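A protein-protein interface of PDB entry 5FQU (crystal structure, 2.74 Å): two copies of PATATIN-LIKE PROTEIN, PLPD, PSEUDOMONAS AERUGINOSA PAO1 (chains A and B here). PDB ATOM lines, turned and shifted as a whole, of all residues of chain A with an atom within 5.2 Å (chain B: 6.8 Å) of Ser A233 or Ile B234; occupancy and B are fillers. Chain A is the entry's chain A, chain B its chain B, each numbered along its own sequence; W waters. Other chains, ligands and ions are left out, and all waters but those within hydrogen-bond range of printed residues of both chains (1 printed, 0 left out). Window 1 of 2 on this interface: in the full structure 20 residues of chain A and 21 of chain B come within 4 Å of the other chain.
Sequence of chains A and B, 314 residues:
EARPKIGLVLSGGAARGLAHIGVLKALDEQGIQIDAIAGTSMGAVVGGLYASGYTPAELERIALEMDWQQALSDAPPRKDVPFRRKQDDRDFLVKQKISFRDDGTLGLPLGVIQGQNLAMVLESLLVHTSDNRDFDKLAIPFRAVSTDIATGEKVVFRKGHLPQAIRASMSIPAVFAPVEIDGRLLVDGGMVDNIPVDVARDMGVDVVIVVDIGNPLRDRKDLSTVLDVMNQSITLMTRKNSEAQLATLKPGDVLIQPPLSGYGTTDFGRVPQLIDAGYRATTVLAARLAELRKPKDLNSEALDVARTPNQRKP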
ATOM      1  N   VAL A 229       4.062 -28.497  14.348  1.00  0.00           N
ATOM      2  CA  VAL A 229       3.276 -27.289  14.556  1.00  0.00           C
ATOM      3  C   VAL A 229       2.810 -26.707  13.222  1.00  0.00           C
ATOM      4  O   VAL A 229       1.709 -26.175  13.116  1.00  0.00           O
ATOM      5  CB  VAL A 229       4.067 -26.238  15.364  1.00  0.00           C
ATOM      6  CG1 VAL A 229       3.336 -24.900  15.390  1.00  0.00           C
ATOM      7  CG2 VAL A 229       4.325 -26.741  16.783  1.00  0.00           C
ATOM      8  N   MET A 230       3.630 -26.851  12.191  1.00  0.00           N
ATOM      9  CA  MET A 230       3.359 -26.167  10.936  1.00  0.00           C
ATOM     10  C   MET A 230       2.417 -26.908  10.060  1.00  0.00           C
ATOM     11  O   MET A 230       1.558 -26.291   9.431  1.00  0.00           O
ATOM     12  CB  MET A 230       4.695 -25.898  10.301  1.00  0.00           C
ATOM     13  CG  MET A 230       5.369 -24.963  11.286  1.00  0.00           C
ATOM     14  SD  MET A 230       6.299 -23.611  10.257  1.00  0.00           S
ATOM     15  CE  MET A 230       8.003 -24.574  10.109  1.00  0.00           C
ATOM     16  N   ASN A 231       2.540 -28.236  10.045  1.00  0.00           N
ATOM     17  CA  ASN A 231       1.477 -29.115   9.526  1.00  0.00           C
ATOM     18  C   ASN A 231       0.109 -28.851  10.116  1.00  0.00           C
ATOM     19  O   ASN A 231      -0.898 -28.879   9.414  1.00  0.00           O
ATOM     20  CB  ASN A 231       1.821 -30.574   9.795  1.00  0.00           C
ATOM     21  CG  ASN A 231       2.863 -31.096   8.843  1.00  0.00           C
ATOM     22  OD1 ASN A 231       2.756 -30.924   7.622  1.00  0.00           O
ATOM     23  ND2 ASN A 231       3.893 -31.716   9.389  1.00  0.00           N
ATOM     24  N   GLN A 232       0.090 -28.620  11.420  1.00  0.00           N
ATOM     25  CA  GLN A 232      -1.129 -28.302  12.137  1.00  0.00           C
ATOM     26  C   GLN A 232      -1.745 -27.018  11.592  1.00  0.00           C
ATOM     27  O   GLN A 232      -2.971 -26.923  11.400  1.00  0.00           O
ATOM     28  CB  GLN A 232      -0.807 -28.160  13.630  1.00  0.00           C
ATOM     29  CG  GLN A 232      -1.980 -27.827  14.537  1.00  0.00           C
ATOM     30  CD  GLN A 232      -2.897 -29.005  14.796  1.00  0.00           C
ATOM     31  OE1 GLN A 232      -2.456 -30.063  15.215  1.00  0.00           O
ATOM     32  NE2 GLN A 232      -4.184 -28.810  14.567  1.00  0.00           N
ATOM     33  N   SER A 233      -0.882 -26.030  11.348  1.00  0.00           N
ATOM     34  CA  SER A 233      -1.310 -24.784  10.757  1.00  0.00           C
ATOM     35  C   SER A 233      -1.955 -25.053   9.392  1.00  0.00           C
ATOM     36  O   SER A 233      -3.099 -24.638   9.134  1.00  0.00           O
ATOM     37  CB  SER A 233      -0.123 -23.855  10.627  1.00  0.00           C
ATOM     38  OG  SER A 233      -0.538 -22.640  10.035  1.00  0.00           O
ATOM     39  N   ILE A 234      -1.260 -25.818   8.546  1.00  0.00           N
ATOM     40  CA  ILE A 234      -1.791 -26.178   7.221  1.00  0.00           C
ATOM     41  C   ILE A 234      -3.130 -26.919   7.351  1.00  0.00           C
ATOM     42  O   ILE A 234      -4.089 -26.652   6.606  1.00  0.00           O
ATOM     43  CB  ILE A 234      -0.807 -27.037   6.415  1.00  0.00           C
ATOM     44  CG1 ILE A 234       0.429 -26.216   6.048  1.00  0.00           C
ATOM     45  CG2 ILE A 234      -1.467 -27.504   5.135  1.00  0.00           C
ATOM     46  CD1 ILE A 234       1.574 -26.997   5.423  1.00  0.00           C
ATOM     47  N   THR A 235      -3.204 -27.829   8.317  1.00  0.00           N
ATOM     48  CA  THR A 235      -4.445 -28.500   8.592  1.00  0.00           C
ATOM     49  C   THR A 235      -5.540 -27.484   8.924  1.00  0.00           C
ATOM     50  O   THR A 235      -6.682 -27.637   8.475  1.00  0.00           O
ATOM     51  CB  THR A 235      -4.302 -29.511   9.731  1.00  0.00           C
ATOM     52  OG1 THR A 235      -3.271 -30.452   9.423  1.00  0.00           O
ATOM     53  CG2 THR A 235      -5.596 -30.256   9.940  1.00  0.00           C
ATOM     54  N   LEU A 236      -5.204 -26.458   9.711  1.00  0.00           N
ATOM     55  CA  LEU A 236      -6.223 -25.505  10.152  1.00  0.00           C
ATOM     56  C   LEU A 236      -6.855 -24.748   8.995  1.00  0.00           C
ATOM     57  O   LEU A 236      -8.078 -24.573   8.978  1.00  0.00           O
ATOM     58  CB  LEU A 236      -5.686 -24.536  11.208  1.00  0.00           C
ATOM     59  CG  LEU A 236      -5.636 -25.155  12.611  1.00  0.00           C
ATOM     60  CD1 LEU A 236      -4.712 -24.371  13.521  1.00  0.00           C
ATOM     61  CD2 LEU A 236      -7.023 -25.252  13.224  1.00  0.00           C
ATOM     62  N   MET A 237      -6.039 -24.329   8.024  1.00  0.00           N
ATOM     63  CA  MET A 237      -6.553 -23.538   6.890  1.00  0.00           C
ATOM     64  C   MET A 237      -7.217 -24.415   5.873  1.00  0.00           C
ATOM     65  O   MET A 237      -8.173 -24.003   5.216  1.00  0.00           O
ATOM     66  CB  MET A 237      -5.499 -22.643   6.226  1.00  0.00           C
ATOM     67  CG  MET A 237      -4.351 -23.374   5.531  1.00  0.00           C
ATOM     68  SD  MET A 237      -3.104 -22.097   4.657  1.00  0.00           S
ATOM     69  CE  MET A 237      -4.278 -21.103   3.405  1.00  0.00           C
ATOM     70  N   THR A 238      -6.708 -25.632   5.733  1.00  0.00           N
ATOM     71  CA  THR A 238      -7.397 -26.682   4.991  1.00  0.00           C
ATOM     72  C   THR A 238      -8.841 -26.967   5.428  1.00  0.00           C
ATOM     73  O   THR A 238      -9.733 -27.106   4.579  1.00  0.00           O
ATOM     74  CB  THR A 238      -6.624 -27.975   5.143  1.00  0.00           C
ATOM     75  OG1 THR A 238      -5.259 -27.724   4.809  1.00  0.00           O
ATOM     76  CG2 THR A 238      -7.200 -29.043   4.247  1.00  0.00           C
ATOM     77  N   ILE B 149      -2.460 -23.994  19.513  1.00  0.00           N
ATOM     78  CA  ILE B 149      -1.970 -24.753  18.391  1.00  0.00           C
ATOM     79  C   ILE B 149      -2.639 -26.126  18.352  1.00  0.00           C
ATOM     80  O   ILE B 149      -2.743 -26.733  17.303  1.00  0.00           O
ATOM     81  CB  ILE B 149      -0.424 -24.815  18.390  1.00  0.00           C
ATOM     82  CG1 ILE B 149       0.090 -25.334  17.055  1.00  0.00           C
ATOM     83  CG2 ILE B 149       0.113 -25.679  19.523  1.00  0.00           C
ATOM     84  CD1 ILE B 149      -0.424 -24.556  15.862  1.00  0.00           C
ATOM     85  N   PRO B 173       6.296 -19.545  15.082  1.00  0.00           N
ATOM     86  CA  PRO B 173       6.836 -20.897  14.896  1.00  0.00           C
ATOM     87  C   PRO B 173       8.127 -20.888  14.089  1.00  0.00           C
ATOM     88  O   PRO B 173       8.280 -20.068  13.163  1.00  0.00           O
ATOM     89  CB  PRO B 173       5.733 -21.621  14.127  1.00  0.00           C
ATOM     90  CG  PRO B 173       4.492 -20.844  14.397  1.00  0.00           C
ATOM     91  CD  PRO B 173       4.938 -19.426  14.522  1.00  0.00           C
ATOM     92  N   ASP B 188       2.230 -17.569  18.216  1.00  0.00           N
ATOM     93  CA  ASP B 188       1.884 -16.362  17.451  1.00  0.00           C
ATOM     94  C   ASP B 188       0.390 -16.375  17.062  1.00  0.00           C
ATOM     95  O   ASP B 188      -0.129 -17.375  16.549  1.00  0.00           O
ATOM     96  CB  ASP B 188       2.823 -16.252  16.213  1.00  0.00           C
ATOM     97  CG  ASP B 188       2.352 -15.214  15.152  1.00  0.00           C
ATOM     98  OD1 ASP B 188       1.976 -14.079  15.523  1.00  0.00           O
ATOM     99  OD2 ASP B 188       2.398 -15.524  13.928  1.00  0.00           O
ATOM    100  N   GLY B 190      -1.000 -14.528  14.849  1.00  0.00           N
ATOM    101  CA  GLY B 190      -1.156 -14.136  13.457  1.00  0.00           C
ATOM    102  C   GLY B 190      -2.017 -15.078  12.644  1.00  0.00           C
ATOM    103  O   GLY B 190      -2.816 -14.641  11.796  1.00  0.00           O
ATOM    104  N   MET B 191      -1.902 -16.377  12.909  1.00  0.00           N
ATOM    105  CA  MET B 191      -2.650 -17.333  12.106  1.00  0.00           C
ATOM    106  C   MET B 191      -4.138 -17.338  12.334  1.00  0.00           C
ATOM    107  O   MET B 191      -4.868 -17.838  11.487  1.00  0.00           O
ATOM    108  CB  MET B 191      -2.079 -18.721  12.161  1.00  0.00           C
ATOM    109  CG  MET B 191      -2.247 -19.489  13.451  1.00  0.00           C
ATOM    110  SD  MET B 191      -0.992 -21.004  13.269  1.00  0.00           S
ATOM    111  CE  MET B 191       0.716 -20.039  13.619  1.00  0.00           C
ATOM    112  N   VAL B 229       8.547 -22.748   2.317  1.00  0.00           N
ATOM    113  CA  VAL B 229       7.224 -23.021   1.770  1.00  0.00           C
ATOM    114  C   VAL B 229       6.169 -22.936   2.869  1.00  0.00           C
ATOM    115  O   VAL B 229       5.043 -22.503   2.630  1.00  0.00           O
ATOM    116  CB  VAL B 229       7.169 -24.393   1.058  1.00  0.00           C
ATOM    117  CG1 VAL B 229       5.739 -24.779   0.679  1.00  0.00           C
ATOM    118  CG2 VAL B 229       8.070 -24.392  -0.175  1.00  0.00           C
ATOM    119  N   MET B 230       6.530 -23.330   4.082  1.00  0.00           N
ATOM    120  CA  MET B 230       5.529 -23.475   5.129  1.00  0.00           C
ATOM    121  C   MET B 230       5.229 -22.196   5.824  1.00  0.00           C
ATOM    122  O   MET B 230       4.071 -21.935   6.142  1.00  0.00           O
ATOM    123  CB  MET B 230       6.007 -24.562   6.047  1.00  0.00           C
ATOM    124  CG  MET B 230       6.003 -25.795   5.165  1.00  0.00           C
ATOM    125  SD  MET B 230       5.320 -27.262   6.240  1.00  0.00           S
ATOM    126  CE  MET B 230       7.092 -27.835   6.914  1.00  0.00           C
ATOM    127  N   ASN B 231       6.260 -21.383   6.036  1.00  0.00           N
ATOM    128  CA  ASN B 231       6.081 -19.965   6.372  1.00  0.00           C
ATOM    129  C   ASN B 231       5.165 -19.230   5.418  1.00  0.00           C
ATOM    130  O   ASN B 231       4.366 -18.400   5.833  1.00  0.00           O
ATOM    131  CB  ASN B 231       7.421 -19.255   6.382  1.00  0.00           C
ATOM    132  CG  ASN B 231       8.207 -19.560   7.622  1.00  0.00           C
ATOM    133  OD1 ASN B 231       7.697 -19.442   8.732  1.00  0.00           O
ATOM    134  ND2 ASN B 231       9.461 -19.958   7.445  1.00  0.00           N
ATOM    135  N   GLN B 232       5.321 -19.523   4.134  1.00  0.00           N
ATOM    136  CA  GLN B 232       4.500 -18.933   3.098  1.00  0.00           C
ATOM    137  C   GLN B 232       3.031 -19.306   3.316  1.00  0.00           C
ATOM    138  O   GLN B 232       2.130 -18.470   3.171  1.00  0.00           O
ATOM    139  CB  GLN B 232       5.000 -19.412   1.727  1.00  0.00           C
ATOM    140  CG  GLN B 232       4.237 -18.904   0.510  1.00  0.00           C
ATOM    141  CD  GLN B 232       4.559 -17.469   0.149  1.00  0.00           C
ATOM    142  OE1 GLN B 232       5.719 -17.092   0.008  1.00  0.00           O
ATOM    143  NE2 GLN B 232       3.521 -16.650   0.023  1.00  0.00           N
ATOM    144  N   SER B 233       2.806 -20.570   3.659  1.00  0.00           N
ATOM    145  CA  SER B 233       1.479 -21.037   3.969  1.00  0.00           C
ATOM    146  C   SER B 233       0.907 -20.239   5.142  1.00  0.00           C
ATOM    147  O   SER B 233      -0.188 -19.680   5.055  1.00  0.00           O
ATOM    148  CB  SER B 233       1.530 -22.518   4.294  1.00  0.00           C
ATOM    149  OG  SER B 233       0.235 -22.985   4.630  1.00  0.00           O
ATOM    150  N   ILE B 234       1.683 -20.142   6.222  1.00  0.00           N
ATOM    151  CA  ILE B 234       1.269 -19.387   7.408  1.00  0.00           C
ATOM    152  C   ILE B 234       0.994 -17.933   7.025  1.00  0.00           C
ATOM    153  O   ILE B 234       0.001 -17.353   7.464  1.00  0.00           O
ATOM    154  CB  ILE B 234       2.325 -19.426   8.531  1.00  0.00           C
ATOM    155  CG1 ILE B 234       2.465 -20.843   9.105  1.00  0.00           C
ATOM    156  CG2 ILE B 234       1.920 -18.485   9.647  1.00  0.00           C
ATOM    157  CD1 ILE B 234       3.613 -21.062  10.080  1.00  0.00           C
ATOM    158  N   THR B 235       1.856 -17.355   6.188  1.00  0.00           N
ATOM    159  CA  THR B 235       1.614 -16.027   5.673  1.00  0.00           C
ATOM    160  C   THR B 235       0.278 -15.957   4.936  1.00  0.00           C
ATOM    161  O   THR B 235      -0.474 -15.005   5.119  1.00  0.00           O
ATOM    162  CB  THR B 235       2.727 -15.571   4.737  1.00  0.00           C
ATOM    163  OG1 THR B 235       3.980 -15.626   5.417  1.00  0.00           O
ATOM    164  CG2 THR B 235       2.487 -14.152   4.290  1.00  0.00           C
ATOM    165  N   LEU B 236      -0.054 -16.984   4.154  1.00  0.00           N
ATOM    166  CA  LEU B 236      -1.290 -16.962   3.374  1.00  0.00           C
ATOM    167  C   LEU B 236      -2.524 -16.911   4.239  1.00  0.00           C
ATOM    168  O   LEU B 236      -3.433 -16.143   3.925  1.00  0.00           O
ATOM    169  CB  LEU B 236      -1.378 -18.132   2.391  1.00  0.00           C
ATOM    170  CG  LEU B 236      -0.549 -17.893   1.125  1.00  0.00           C
ATOM    171  CD1 LEU B 236      -0.287 -19.199   0.401  1.00  0.00           C
ATOM    172  CD2 LEU B 236      -1.215 -16.892   0.189  1.00  0.00           C
ATOM    173  N   MET B 237      -2.555 -17.706   5.319  1.00  0.00           N
ATOM    174  CA  MET B 237      -3.740 -17.765   6.201  1.00  0.00           C
ATOM    175  C   MET B 237      -3.802 -16.585   7.124  1.00  0.00           C
ATOM    176  O   MET B 237      -4.885 -16.100   7.454  1.00  0.00           O
ATOM    177  CB  MET B 237      -3.890 -19.051   7.012  1.00  0.00           C
ATOM    178  CG  MET B 237      -2.800 -19.291   8.053  1.00  0.00           C
ATOM    179  SD  MET B 237      -3.128 -20.957   9.058  1.00  0.00           S
ATOM    180  CE  MET B 237      -4.918 -20.657   9.858  1.00  0.00           C
ATOM    181  N   THR B 238      -2.636 -16.100   7.536  1.00  0.00           N
ATOM    182  CA  THR B 238      -2.510 -14.798   8.175  1.00  0.00           C
ATOM    183  C   THR B 238      -3.148 -13.632   7.412  1.00  0.00           C
ATOM    184  O   THR B 238      -3.830 -12.793   8.024  1.00  0.00           O
ATOM    185  CB  THR B 238      -1.043 -14.474   8.361  1.00  0.00           C
ATOM    186  OG1 THR B 238      -0.443 -15.585   9.009  1.00  0.00           O
ATOM    187  CG2 THR B 238      -0.866 -13.233   9.200  1.00  0.00           C
ATOM    188  N   ARG B 239      -2.874 -13.547   6.107  1.00  0.00           N
ATOM    189  CA  ARG B 239      -3.460 -12.505   5.268  1.00  0.00           C
ATOM    190  C   ARG B 239      -4.964 -12.684   5.120  1.00  0.00           C
ATOM    191  O   ARG B 239      -5.705 -11.707   5.081  1.00  0.00           O
ATOM    192  CB  ARG B 239      -2.831 -12.504   3.893  1.00  0.00           C
ATOM    193  CG  ARG B 239      -1.422 -11.957   3.858  1.00  0.00           C
ATOM    194  CD  ARG B 239      -0.756 -12.363   2.553  1.00  0.00           C
ATOM    195  NE  ARG B 239      -1.170 -11.508   1.435  1.00  0.00           N
ATOM    196  CZ  ARG B 239      -0.534 -10.399   1.048  1.00  0.00           C
ATOM    197  NH1 ARG B 239       0.570  -9.978   1.666  1.00  0.00           N
ATOM    198  NH2 ARG B 239      -0.996  -9.709   0.013  1.00  0.00           N
ATOM    199  N   ASN B 241      -7.241 -14.066   7.241  1.00  0.00           N
ATOM    200  CA  ASN B 241      -7.939 -13.546   8.448  1.00  0.00           C
ATOM    201  C   ASN B 241      -7.746 -12.034   8.623  1.00  0.00           C
ATOM    202  O   ASN B 241      -8.577 -11.353   9.231  1.00  0.00           O
ATOM    203  CB  ASN B 241      -7.530 -14.309   9.731  1.00  0.00           C
ATOM    204  CG  ASN B 241      -6.163 -13.877  10.289  1.00  0.00           C
ATOM    205  OD1 ASN B 241      -5.968 -12.711  10.661  1.00  0.00           O
ATOM    206  ND2 ASN B 241      -5.235 -14.830  10.410  1.00  0.00           N
HETATM  207  O   HOH W   1      -0.304 -22.752   7.261  1.00  0.00           O
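Met A230 touches Ile B234, and with the chains exchanged Ile A234 touches Met B230. Ser A233 touches Ile B234, and with the chains exchanged Ile A234 touches Ser B233. Ser A233 touches Met B237, and with the chains exchanged Met A237 touches Ser B233. Met B237 touches its own counterpart, Met A237. Of the 10 pairs that touch across the chains among the printed residues, 7 have their exchanged pair printed and touching as well.
O of Met B191 is in hydrogen-bond range of ND2 of Asn B241, at 3.2 Å. O of Met B237 sits at hydrogen-bond distance from ND2 of Asn B241 (3.2 Å).
The side-chain sulfur (SD) of Met B191 is in hydrogen-bond range of the side-chain hydroxyl (OG) of Ser A233, 3.7 Å away. The side-chain sulfur of Met B237 sits at hydrogen-bond distance from the side-chain hydroxyl of Ser A233. The side-chain sulfur (SD) of Met A237 lies within hydrogen-bond range of the side-chain hydroxyl (OG) of Ser B233, at 3.5 Å.
Ser A233 touches three residues of chain B. Ile B234 touches just these residues of chain A: Met A230 (3.7 Å) and Ser A233 (3.6 Å). Of the printed residues of chain A, Ile B149 touches Val A229 and Gln A232. Printed residues of chain B within 4 Å of Met A237: Ser B233 and Met B237. Of the printed residues of chain A, Ser B233 touches Ile A234 and Met A237. Pro B173 touches none of the printed residues of chain A. Asn B231 touches none of the printed residues of chain A. The nearest residue of chain B that does not touch Ser A233 is Ile B149 (4.8 Å). The nearest printed residue of chain A that does not touch Ile B234 is Met A237 (5.4 Å). The nearest printed residue of chain B that does not touch Met A237 is Leu B236 (4.3 Å).
CG1 of Val A229 touches CG1 of Ile B149, at 3.7 Å. Ile B234 touches Met A230 (CD1 to SD, 3.7 Å). CG of Gln A232 touches O of Ile B149, at 3.1 Å. Ser A233 touches Ile B234. Ile A234 touches Met B230 (CD1 to SD, 3.8 Å). Ile A234 touches Ser B233. Met A237 touches Met B237 (SD to CB, 3.9 Å).
Of the 17 printed residues of chain B, 6 touch a printed residue of chain A. Hydrophobic or aromatic side chains of chain B that line the printed part of chain A: Ile B149, Met B191, Met B230, Ile B234 and Met B237. Along chain B the printed residues that touch a printed residue of chain A span positions 149 to 237. Among the printed residues, no Asp or Glu carboxylate lies within 4 Å of a Lys or Arg side-chain nitrogen of the other chain.
Water W1 lies within hydrogen-bond range of OG of Ser B233, OG of Ser A233, N of Ile B234, N of Ile A234 and SD of Met B237.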
